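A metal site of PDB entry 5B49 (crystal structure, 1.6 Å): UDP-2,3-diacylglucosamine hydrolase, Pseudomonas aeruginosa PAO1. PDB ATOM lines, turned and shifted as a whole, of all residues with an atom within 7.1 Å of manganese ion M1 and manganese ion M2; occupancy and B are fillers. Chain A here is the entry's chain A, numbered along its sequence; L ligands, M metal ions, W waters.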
ATOM      1  N   SER A   7      27.730 -24.008  -6.536  1.00  0.00           N
ATOM      2  CA  SER A   7      27.898 -24.239  -7.971  1.00  0.00           C
ATOM      3  C   SER A   7      28.852 -23.205  -8.500  1.00  0.00           C
ATOM      4  O   SER A   7      29.171 -22.213  -7.849  1.00  0.00           O
ATOM      5  CB  SER A   7      26.581 -24.181  -8.752  1.00  0.00           C
ATOM      6  OG  SER A   7      26.027 -22.896  -8.758  1.00  0.00           O
ATOM      7  N   ASP A   8      29.276 -23.399  -9.755  1.00  0.00           N
ATOM      8  CA  ASP A   8      29.969 -22.343 -10.491  1.00  0.00           C
ATOM      9  C   ASP A   8      31.238 -21.910  -9.757  1.00  0.00           C
ATOM     10  O   ASP A   8      31.540 -20.720  -9.585  1.00  0.00           O
ATOM     11  CB  ASP A   8      29.025 -21.169 -10.786  1.00  0.00           C
ATOM     12  CG  ASP A   8      27.884 -21.569 -11.699  1.00  0.00           C
ATOM     13  OD1 ASP A   8      28.106 -21.698 -12.935  1.00  0.00           O
ATOM     14  OD2 ASP A   8      26.762 -21.783 -11.183  1.00  0.00           O
ATOM     15  N   LEU A   9      32.002 -22.918  -9.326  1.00  0.00           N
ATOM     16  CA  LEU A   9      33.317 -22.670  -8.762  1.00  0.00           C
ATOM     17  C   LEU A   9      34.379 -22.548  -9.858  1.00  0.00           C
ATOM     18  O   LEU A   9      35.328 -21.788  -9.693  1.00  0.00           O
ATOM     19  CB  LEU A   9      33.720 -23.782  -7.792  1.00  0.00           C
ATOM     20  CG  LEU A   9      32.986 -23.812  -6.454  1.00  0.00           C
ATOM     21  CD1 LEU A   9      31.609 -24.444  -6.584  1.00  0.00           C
ATOM     22  CD2 LEU A   9      33.804 -24.583  -5.436  1.00  0.00           C
ATOM     23  N   HIS A  10      34.218 -23.307 -10.961  1.00  0.00           N
ATOM     24  CA  HIS A  10      35.161 -23.299 -12.087  1.00  0.00           C
ATOM     25  C   HIS A  10      36.588 -23.565 -11.616  1.00  0.00           C
ATOM     26  O   HIS A  10      37.532 -22.889 -12.033  1.00  0.00           O
ATOM     27  CB  HIS A  10      35.081 -21.974 -12.857  1.00  0.00           C
ATOM     28  CG  HIS A  10      33.663 -21.483 -13.051  1.00  0.00           C
ATOM     29  ND1 HIS A  10      33.143 -20.443 -12.325  1.00  0.00           N
ATOM     30  CD2 HIS A  10      32.645 -21.941 -13.824  1.00  0.00           C
ATOM     31  CE1 HIS A  10      31.877 -20.239 -12.672  1.00  0.00           C
ATOM     32  NE2 HIS A  10      31.547 -21.157 -13.564  1.00  0.00           N
ATOM     33  N   LEU A  39      25.957 -28.004  -7.942  1.00  0.00           N
ATOM     34  CA  LEU A  39      25.038 -27.949  -9.083  1.00  0.00           C
ATOM     35  C   LEU A  39      25.717 -27.436 -10.341  1.00  0.00           C
ATOM     36  O   LEU A  39      25.232 -26.499 -11.009  1.00  0.00           O
ATOM     37  CB  LEU A  39      23.815 -27.112  -8.741  1.00  0.00           C
ATOM     38  CG  LEU A  39      23.034 -27.577  -7.506  1.00  0.00           C
ATOM     39  CD1 LEU A  39      21.748 -26.743  -7.379  1.00  0.00           C
ATOM     40  CD2 LEU A  39      22.715 -29.071  -7.535  1.00  0.00           C
ATOM     41  N   GLY A  40      26.812 -28.063 -10.731  1.00  0.00           N
ATOM     42  CA  GLY A  40      27.388 -27.845 -12.049  1.00  0.00           C
ATOM     43  C   GLY A  40      28.460 -26.774 -12.058  1.00  0.00           C
ATOM     44  O   GLY A  40      28.522 -25.890 -11.211  1.00  0.00           O
ATOM     45  N   ASP A  41      29.309 -26.857 -13.071  1.00  0.00           N
ATOM     46  CA  ASP A  41      30.432 -25.927 -13.277  1.00  0.00           C
ATOM     47  C   ASP A  41      31.343 -25.960 -12.051  1.00  0.00           C
ATOM     48  O   ASP A  41      31.821 -24.920 -11.557  1.00  0.00           O
ATOM     49  CB  ASP A  41      29.965 -24.520 -13.590  1.00  0.00           C
ATOM     50  CG  ASP A  41      29.428 -24.361 -15.019  1.00  0.00           C
ATOM     51  OD1 ASP A  41      29.323 -25.372 -15.753  1.00  0.00           O
ATOM     52  OD2 ASP A  41      29.083 -23.216 -15.344  1.00  0.00           O
ATOM     53  N   PHE A  42      31.532 -27.172 -11.530  1.00  0.00           N
ATOM     54  CA  PHE A  42      32.447 -27.394 -10.415  1.00  0.00           C
ATOM     55  C   PHE A  42      33.884 -27.164 -10.843  1.00  0.00           C
ATOM     56  O   PHE A  42      34.653 -26.484 -10.152  1.00  0.00           O
ATOM     57  CB  PHE A  42      32.224 -28.807  -9.883  1.00  0.00           C
ATOM     58  CG  PHE A  42      33.039 -29.185  -8.685  1.00  0.00           C
ATOM     59  CD1 PHE A  42      33.059 -28.399  -7.533  1.00  0.00           C
ATOM     60  CD2 PHE A  42      33.702 -30.379  -8.669  1.00  0.00           C
ATOM     61  CE1 PHE A  42      33.780 -28.799  -6.409  1.00  0.00           C
ATOM     62  CE2 PHE A  42      34.430 -30.802  -7.547  1.00  0.00           C
ATOM     63  CZ  PHE A  42      34.453 -30.008  -6.416  1.00  0.00           C
ATOM     64  N   GLY A  78      27.360 -29.473 -15.032  1.00  0.00           N
ATOM     65  CA  GLY A  78      27.114 -28.165 -15.613  1.00  0.00           C
ATOM     66  C   GLY A  78      27.564 -28.121 -17.048  1.00  0.00           C
ATOM     67  O   GLY A  78      27.942 -29.149 -17.614  1.00  0.00           O
ATOM     68  N   ASN A  79      27.581 -26.965 -17.667  1.00  0.00           N
ATOM     69  CA  ASN A  79      27.978 -26.983 -19.057  1.00  0.00           C
ATOM     70  C   ASN A  79      29.489 -27.028 -19.228  1.00  0.00           C
ATOM     71  O   ASN A  79      29.953 -27.372 -20.316  1.00  0.00           O
ATOM     72  CB  ASN A  79      27.375 -25.801 -19.782  1.00  0.00           C
ATOM     73  CG  ASN A  79      27.723 -24.530 -19.149  1.00  0.00           C
ATOM     74  OD1 ASN A  79      27.207 -24.209 -18.079  1.00  0.00           O
ATOM     75  ND2 ASN A  79      28.643 -23.814 -19.749  1.00  0.00           N
ATOM     76  N   ARG A  80      30.254 -26.760 -18.174  1.00  0.00           N
ATOM     77  CA  ARG A  80      31.701 -26.940 -18.228  1.00  0.00           C
ATOM     78  C   ARG A  80      32.110 -28.382 -18.031  1.00  0.00           C
ATOM     79  O   ARG A  80      33.174 -28.790 -18.521  1.00  0.00           O
ATOM     80  CB  ARG A  80      32.396 -26.105 -17.151  1.00  0.00           C
ATOM     81  CG  ARG A  80      32.229 -24.640 -17.312  1.00  0.00           C
ATOM     82  CD  ARG A  80      32.793 -24.133 -18.617  1.00  0.00           C
ATOM     83  NE  ARG A  80      32.716 -22.678 -18.627  1.00  0.00           N
ATOM     84  CZ  ARG A  80      33.549 -21.866 -17.995  1.00  0.00           C
ATOM     85  NH1 ARG A  80      34.594 -22.333 -17.298  1.00  0.00           N
ATOM     86  NH2 ARG A  80      33.341 -20.554 -18.034  1.00  0.00           N
ATOM     87  N   HIS A 114      21.470 -27.304 -13.242  1.00  0.00           N
ATOM     88  CA  HIS A 114      22.545 -26.345 -13.381  1.00  0.00           C
ATOM     89  C   HIS A 114      21.989 -24.970 -13.751  1.00  0.00           C
ATOM     90  O   HIS A 114      22.430 -23.965 -13.205  1.00  0.00           O
ATOM     91  CB  HIS A 114      23.587 -26.802 -14.394  1.00  0.00           C
ATOM     92  CG  HIS A 114      24.690 -25.794 -14.588  1.00  0.00           C
ATOM     93  ND1 HIS A 114      25.455 -25.329 -13.549  1.00  0.00           N
ATOM     94  CD2 HIS A 114      25.084 -25.100 -15.680  1.00  0.00           C
ATOM     95  CE1 HIS A 114      26.303 -24.418 -13.988  1.00  0.00           C
ATOM     96  NE2 HIS A 114      26.096 -24.265 -15.286  1.00  0.00           N
ATOM     97  N   GLY A 115      21.020 -24.925 -14.657  1.00  0.00           N
ATOM     98  CA  GLY A 115      20.370 -23.676 -15.014  1.00  0.00           C
ATOM     99  C   GLY A 115      20.480 -23.330 -16.483  1.00  0.00           C
ATOM    100  O   GLY A 115      19.633 -22.570 -16.991  1.00  0.00           O
ATOM    101  N   ASP A 116      21.475 -23.866 -17.180  1.00  0.00           N
ATOM    102  CA  ASP A 116      21.674 -23.452 -18.574  1.00  0.00           C
ATOM    103  C   ASP A 116      20.554 -23.969 -19.461  1.00  0.00           C
ATOM    104  O   ASP A 116      20.269 -23.356 -20.482  1.00  0.00           O
ATOM    105  CB  ASP A 116      23.023 -23.932 -19.092  1.00  0.00           C
ATOM    106  CG  ASP A 116      23.148 -25.418 -19.091  1.00  0.00           C
ATOM    107  OD1 ASP A 116      22.982 -26.031 -18.011  1.00  0.00           O
ATOM    108  OD2 ASP A 116      23.441 -26.001 -20.174  1.00  0.00           O
ATOM    109  N   TYR A 125      23.218 -20.994 -28.196  1.00  0.00           N
ATOM    110  CA  TYR A 125      23.629 -21.911 -27.140  1.00  0.00           C
ATOM    111  C   TYR A 125      22.718 -23.128 -27.097  1.00  0.00           C
ATOM    112  O   TYR A 125      23.193 -24.257 -26.912  1.00  0.00           O
ATOM    113  CB  TYR A 125      23.650 -21.208 -25.773  1.00  0.00           C
ATOM    114  CG  TYR A 125      23.957 -22.261 -24.729  1.00  0.00           C
ATOM    115  CD1 TYR A 125      25.157 -22.938 -24.780  1.00  0.00           C
ATOM    116  CD2 TYR A 125      23.002 -22.653 -23.796  1.00  0.00           C
ATOM    117  CE1 TYR A 125      25.441 -23.964 -23.914  1.00  0.00           C
ATOM    118  CE2 TYR A 125      23.286 -23.692 -22.901  1.00  0.00           C
ATOM    119  CZ  TYR A 125      24.509 -24.340 -22.981  1.00  0.00           C
ATOM    120  OH  TYR A 125      24.849 -25.372 -22.136  1.00  0.00           O
ATOM    121  N   GLY A 194      22.216 -22.864 -10.670  1.00  0.00           N
ATOM    122  CA  GLY A 194      23.309 -21.929 -10.816  1.00  0.00           C
ATOM    123  C   GLY A 194      23.362 -21.392 -12.226  1.00  0.00           C
ATOM    124  O   GLY A 194      22.362 -20.859 -12.740  1.00  0.00           O
ATOM    125  N   HIS A 195      24.535 -21.518 -12.865  1.00  0.00           N
ATOM    126  CA  HIS A 195      24.816 -21.159 -14.257  1.00  0.00           C
ATOM    127  C   HIS A 195      24.857 -19.656 -14.528  1.00  0.00           C
ATOM    128  O   HIS A 195      25.783 -19.194 -15.191  1.00  0.00           O
ATOM    129  CB  HIS A 195      23.835 -21.786 -15.259  1.00  0.00           C
ATOM    130  CG  HIS A 195      24.171 -21.432 -16.671  1.00  0.00           C
ATOM    131  ND1 HIS A 195      25.353 -21.831 -17.279  1.00  0.00           N
ATOM    132  CD2 HIS A 195      23.535 -20.654 -17.582  1.00  0.00           C
ATOM    133  CE1 HIS A 195      25.411 -21.319 -18.503  1.00  0.00           C
ATOM    134  NE2 HIS A 195      24.308 -20.623 -18.710  1.00  0.00           N
ATOM    135  N   THR A 196      23.846 -18.903 -14.090  1.00  0.00           N
ATOM    136  CA  THR A 196      23.727 -17.510 -14.528  1.00  0.00           C
ATOM    137  C   THR A 196      24.623 -16.545 -13.769  1.00  0.00           C
ATOM    138  O   THR A 196      24.746 -15.398 -14.194  1.00  0.00           O
ATOM    139  CB  THR A 196      22.280 -17.036 -14.404  1.00  0.00           C
ATOM    140  OG1 THR A 196      21.885 -17.095 -13.043  1.00  0.00           O
ATOM    141  CG2 THR A 196      21.352 -17.890 -15.271  1.00  0.00           C
ATOM    142  N   HIS A 197      25.236 -16.986 -12.665  1.00  0.00           N
ATOM    143  CA  HIS A 197      26.193 -16.183 -11.904  1.00  0.00           C
ATOM    144  C   HIS A 197      25.532 -14.910 -11.351  1.00  0.00           C
ATOM    145  O   HIS A 197      26.168 -13.876 -11.196  1.00  0.00           O
ATOM    146  CB  HIS A 197      27.415 -15.795 -12.729  1.00  0.00           C
ATOM    147  CG  HIS A 197      28.238 -16.956 -13.197  1.00  0.00           C
ATOM    148  ND1 HIS A 197      29.467 -16.780 -13.817  1.00  0.00           N
ATOM    149  CD2 HIS A 197      28.034 -18.295 -13.162  1.00  0.00           C
ATOM    150  CE1 HIS A 197      29.972 -17.961 -14.128  1.00  0.00           C
ATOM    151  NE2 HIS A 197      29.124 -18.897 -13.737  1.00  0.00           N
ATOM    152  N   ASP A 218      28.568 -17.550  -8.243  1.00  0.00           N
ATOM    153  CA  ASP A 218      29.828 -18.064  -8.760  1.00  0.00           C
ATOM    154  C   ASP A 218      30.971 -17.554  -7.896  1.00  0.00           C
ATOM    155  O   ASP A 218      30.839 -16.549  -7.190  1.00  0.00           O
ATOM    156  CB  ASP A 218      30.034 -17.621 -10.199  1.00  0.00           C
ATOM    157  CG  ASP A 218      30.311 -16.137 -10.302  1.00  0.00           C
ATOM    158  OD1 ASP A 218      29.353 -15.354 -10.125  1.00  0.00           O
ATOM    159  OD2 ASP A 218      31.472 -15.767 -10.528  1.00  0.00           O
HETATM  160  O1  LIG L   1      30.361 -21.933 -19.970  1.00  0.00           O
HETATM  161  P1  LIG L   1      29.822 -20.569 -19.623  1.00  0.00           P
HETATM  162  O2  LIG L   1      28.811 -20.627 -18.522  1.00  0.00           O
HETATM  163  O3  LIG L   1      30.854 -19.481 -19.516  1.00  0.00           O
HETATM  164  O4  LIG L   1      29.036 -20.092 -20.991  1.00  0.00           O
HETATM  165  C1  LIG L   1      27.898 -20.859 -21.366  1.00  0.00           C
HETATM  166  C2  LIG L   1      27.897 -21.142 -22.864  1.00  0.00           C
HETATM  167  N1  LIG L   1      29.129 -21.804 -23.307  1.00  0.00           N
HETATM  168  C3  LIG L   1      29.317 -23.112 -23.212  1.00  0.00           C
HETATM  169  C4  LIG L   1      30.670 -23.598 -23.746  1.00  0.00           C
HETATM  170  C5  LIG L   1      31.565 -24.027 -22.578  1.00  0.00           C
HETATM  171  O5  LIG L   1      32.044 -22.843 -21.976  1.00  0.00           O
HETATM  172  C6  LIG L   1      32.765 -24.863 -23.065  1.00  0.00           C
HETATM  173  C7  LIG L   1      33.110 -25.993 -22.073  1.00  0.00           C
HETATM  174  C8  LIG L   1      34.052 -27.063 -22.616  1.00  0.00           C
HETATM  175  C9  LIG L   1      33.924 -28.409 -21.881  1.00  0.00           C
HETATM  176  C10 LIG L   1      33.540 -29.583 -22.770  1.00  0.00           C
HETATM  177  C11 LIG L   1      34.665 -30.065 -23.671  1.00  0.00           C
HETATM  178  C12 LIG L   1      34.080 -30.932 -24.791  1.00  0.00           C
HETATM  179  C13 LIG L   1      34.993 -31.077 -25.987  1.00  0.00           C
HETATM  180  C14 LIG L   1      36.373 -31.567 -25.615  1.00  0.00           C
HETATM  181  C15 LIG L   1      36.336 -32.779 -24.700  1.00  0.00           C
HETATM  182  C16 LIG L   1      35.558 -33.930 -25.278  1.00  0.00           C
HETATM  183  O6  LIG L   1      28.480 -23.867 -22.778  1.00  0.00           O
HETATM  184  C17 LIG L   1      27.703 -19.877 -23.661  1.00  0.00           C
HETATM  185  C18 LIG L   1      26.523 -19.095 -23.139  1.00  0.00           C
HETATM  186  C19 LIG L   1      26.643 -18.871 -21.653  1.00  0.00           C
HETATM  187  O7  LIG L   1      26.746 -20.124 -20.983  1.00  0.00           O
HETATM  188  C20 LIG L   1      25.432 -18.133 -21.061  1.00  0.00           C
HETATM  189  O8  LIG L   1      24.268 -18.999 -21.031  1.00  0.00           O
HETATM  190  O9  LIG L   1      26.507 -17.817 -23.813  1.00  0.00           O
HETATM  191  O10 LIG L   1      27.391 -20.340 -24.947  1.00  0.00           O
HETATM  192  C21 LIG L   1      28.011 -19.746 -26.073  1.00  0.00           C
HETATM  193  O11 LIG L   1      28.612 -18.684 -25.962  1.00  0.00           O
HETATM  194  C22 LIG L   1      27.869 -20.527 -27.345  1.00  0.00           C
HETATM  195  C23 LIG L   1      27.961 -19.668 -28.590  1.00  0.00           C
HETATM  196  O12 LIG L   1      26.761 -18.864 -28.626  1.00  0.00           O
HETATM  197  C24 LIG L   1      28.063 -20.539 -29.851  1.00  0.00           C
HETATM  198  C25 LIG L   1      29.429 -21.167 -29.957  1.00  0.00           C
HETATM  199  C26 LIG L   1      29.621 -22.144 -31.127  1.00  0.00           C
HETATM  200  C27 LIG L   1      31.091 -22.582 -31.088  1.00  0.00           C
HETATM  201  C28 LIG L   1      31.488 -23.598 -32.136  1.00  0.00           C
HETATM  202  C29 LIG L   1      32.985 -23.852 -32.046  1.00  0.00           C
HETATM  203  C30 LIG L   1      33.534 -24.915 -32.994  1.00  0.00           C
HETATM  204  C31 LIG L   1      33.230 -24.545 -34.427  1.00  0.00           C
HETATM  205  C32 LIG L   1      34.203 -25.228 -35.369  1.00  0.00           C
HETATM  206  C33 LIG L   1      33.622 -25.401 -36.778  1.00  0.00           C
HETATM  207  C34 LIG L   1      34.722 -25.423 -37.798  1.00  0.00           C
HETATM  208 MN    MN M   1      27.261 -22.819 -16.508  1.00  0.00          MN
HETATM  209 MN    MN M   2      29.491 -21.074 -14.481  1.00  0.00          MN
HETATM  210  O   HOH W   1      27.807 -20.767 -15.962  1.00  0.00           O
HETATM  211  O   HOH W   2      30.731 -20.397 -16.221  1.00  0.00           O
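ND2 of Asn 79 is in hydrogen-bond range of O1 of the ligand (2.6 Å). NE2 of His 195 sits at hydrogen-bond distance from O8 of the ligand (2.8 Å). The guanidinium group of Arg 80 is in salt-bridge range of an oxygen (O1) of the ligand (2.8 Å).
Manganese ion M2 is bound by OD1 of Asp 8, water W2, NE2 of His 10, water W1, NE2 of His 197 and OD2 of Asp 41.
Manganese ion M1 is bound by the side-chain amide oxygen of Asn 79 (2.1 Å), water W1 (2.2 Å), the side-chain carboxylate of Asp 41 (2.2 Å), a ring nitrogen (NE2) of His 114 (2.2 Å) and a ring nitrogen (ND1) of His 195 (2.3 Å). Manganese ion M1 has five donor atoms within binding distance.
Within 4 Å of manganese ion M2: Asp 8, His 10, Asp 41 and His 197.
Water W1 lies within hydrogen-bond range of the backbone carbonyl oxygen (O) of His 195 (2.7 Å) and an oxygen (O2) of the ligand (2.8 Å). Water W2 bridges O2 of the ligand (3.0 Å) and NH2 of Arg 80 (3.2 Å).
The backbone NH (N) of His 195 lies within hydrogen-bond range of the side-chain carboxylate (OD2) of Asp 8. The backbone carbonyl oxygen (O) of Gly 40 sits at hydrogen-bond distance from the backbone NH (N) of Asp 8, at 3.0 Å. OG of Ser 7 is in hydrogen-bond range of OD2 of Asp 8, at 2.8 Å. The side-chain carboxylate (OD1) of Asp 41 is in hydrogen-bond range of the backbone NH (N) of Arg 80 (2.9 Å). The backbone carbonyl oxygen of Asp 41 lies within hydrogen-bond range of the backbone NH of Leu 9 (3.0 Å). The backbone carbonyl oxygen (O) of His 114 lies within hydrogen-bond range of the backbone NH (N) of Gly 194. The backbone carbonyl oxygen (O) of Leu 39 is in hydrogen-bond range of a ring nitrogen (ND1) of His 114 (2.8 Å). The backbone NH of His 10 is in hydrogen-bond range of the backbone carbonyl oxygen of Phe 42, 3.3 Å away.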
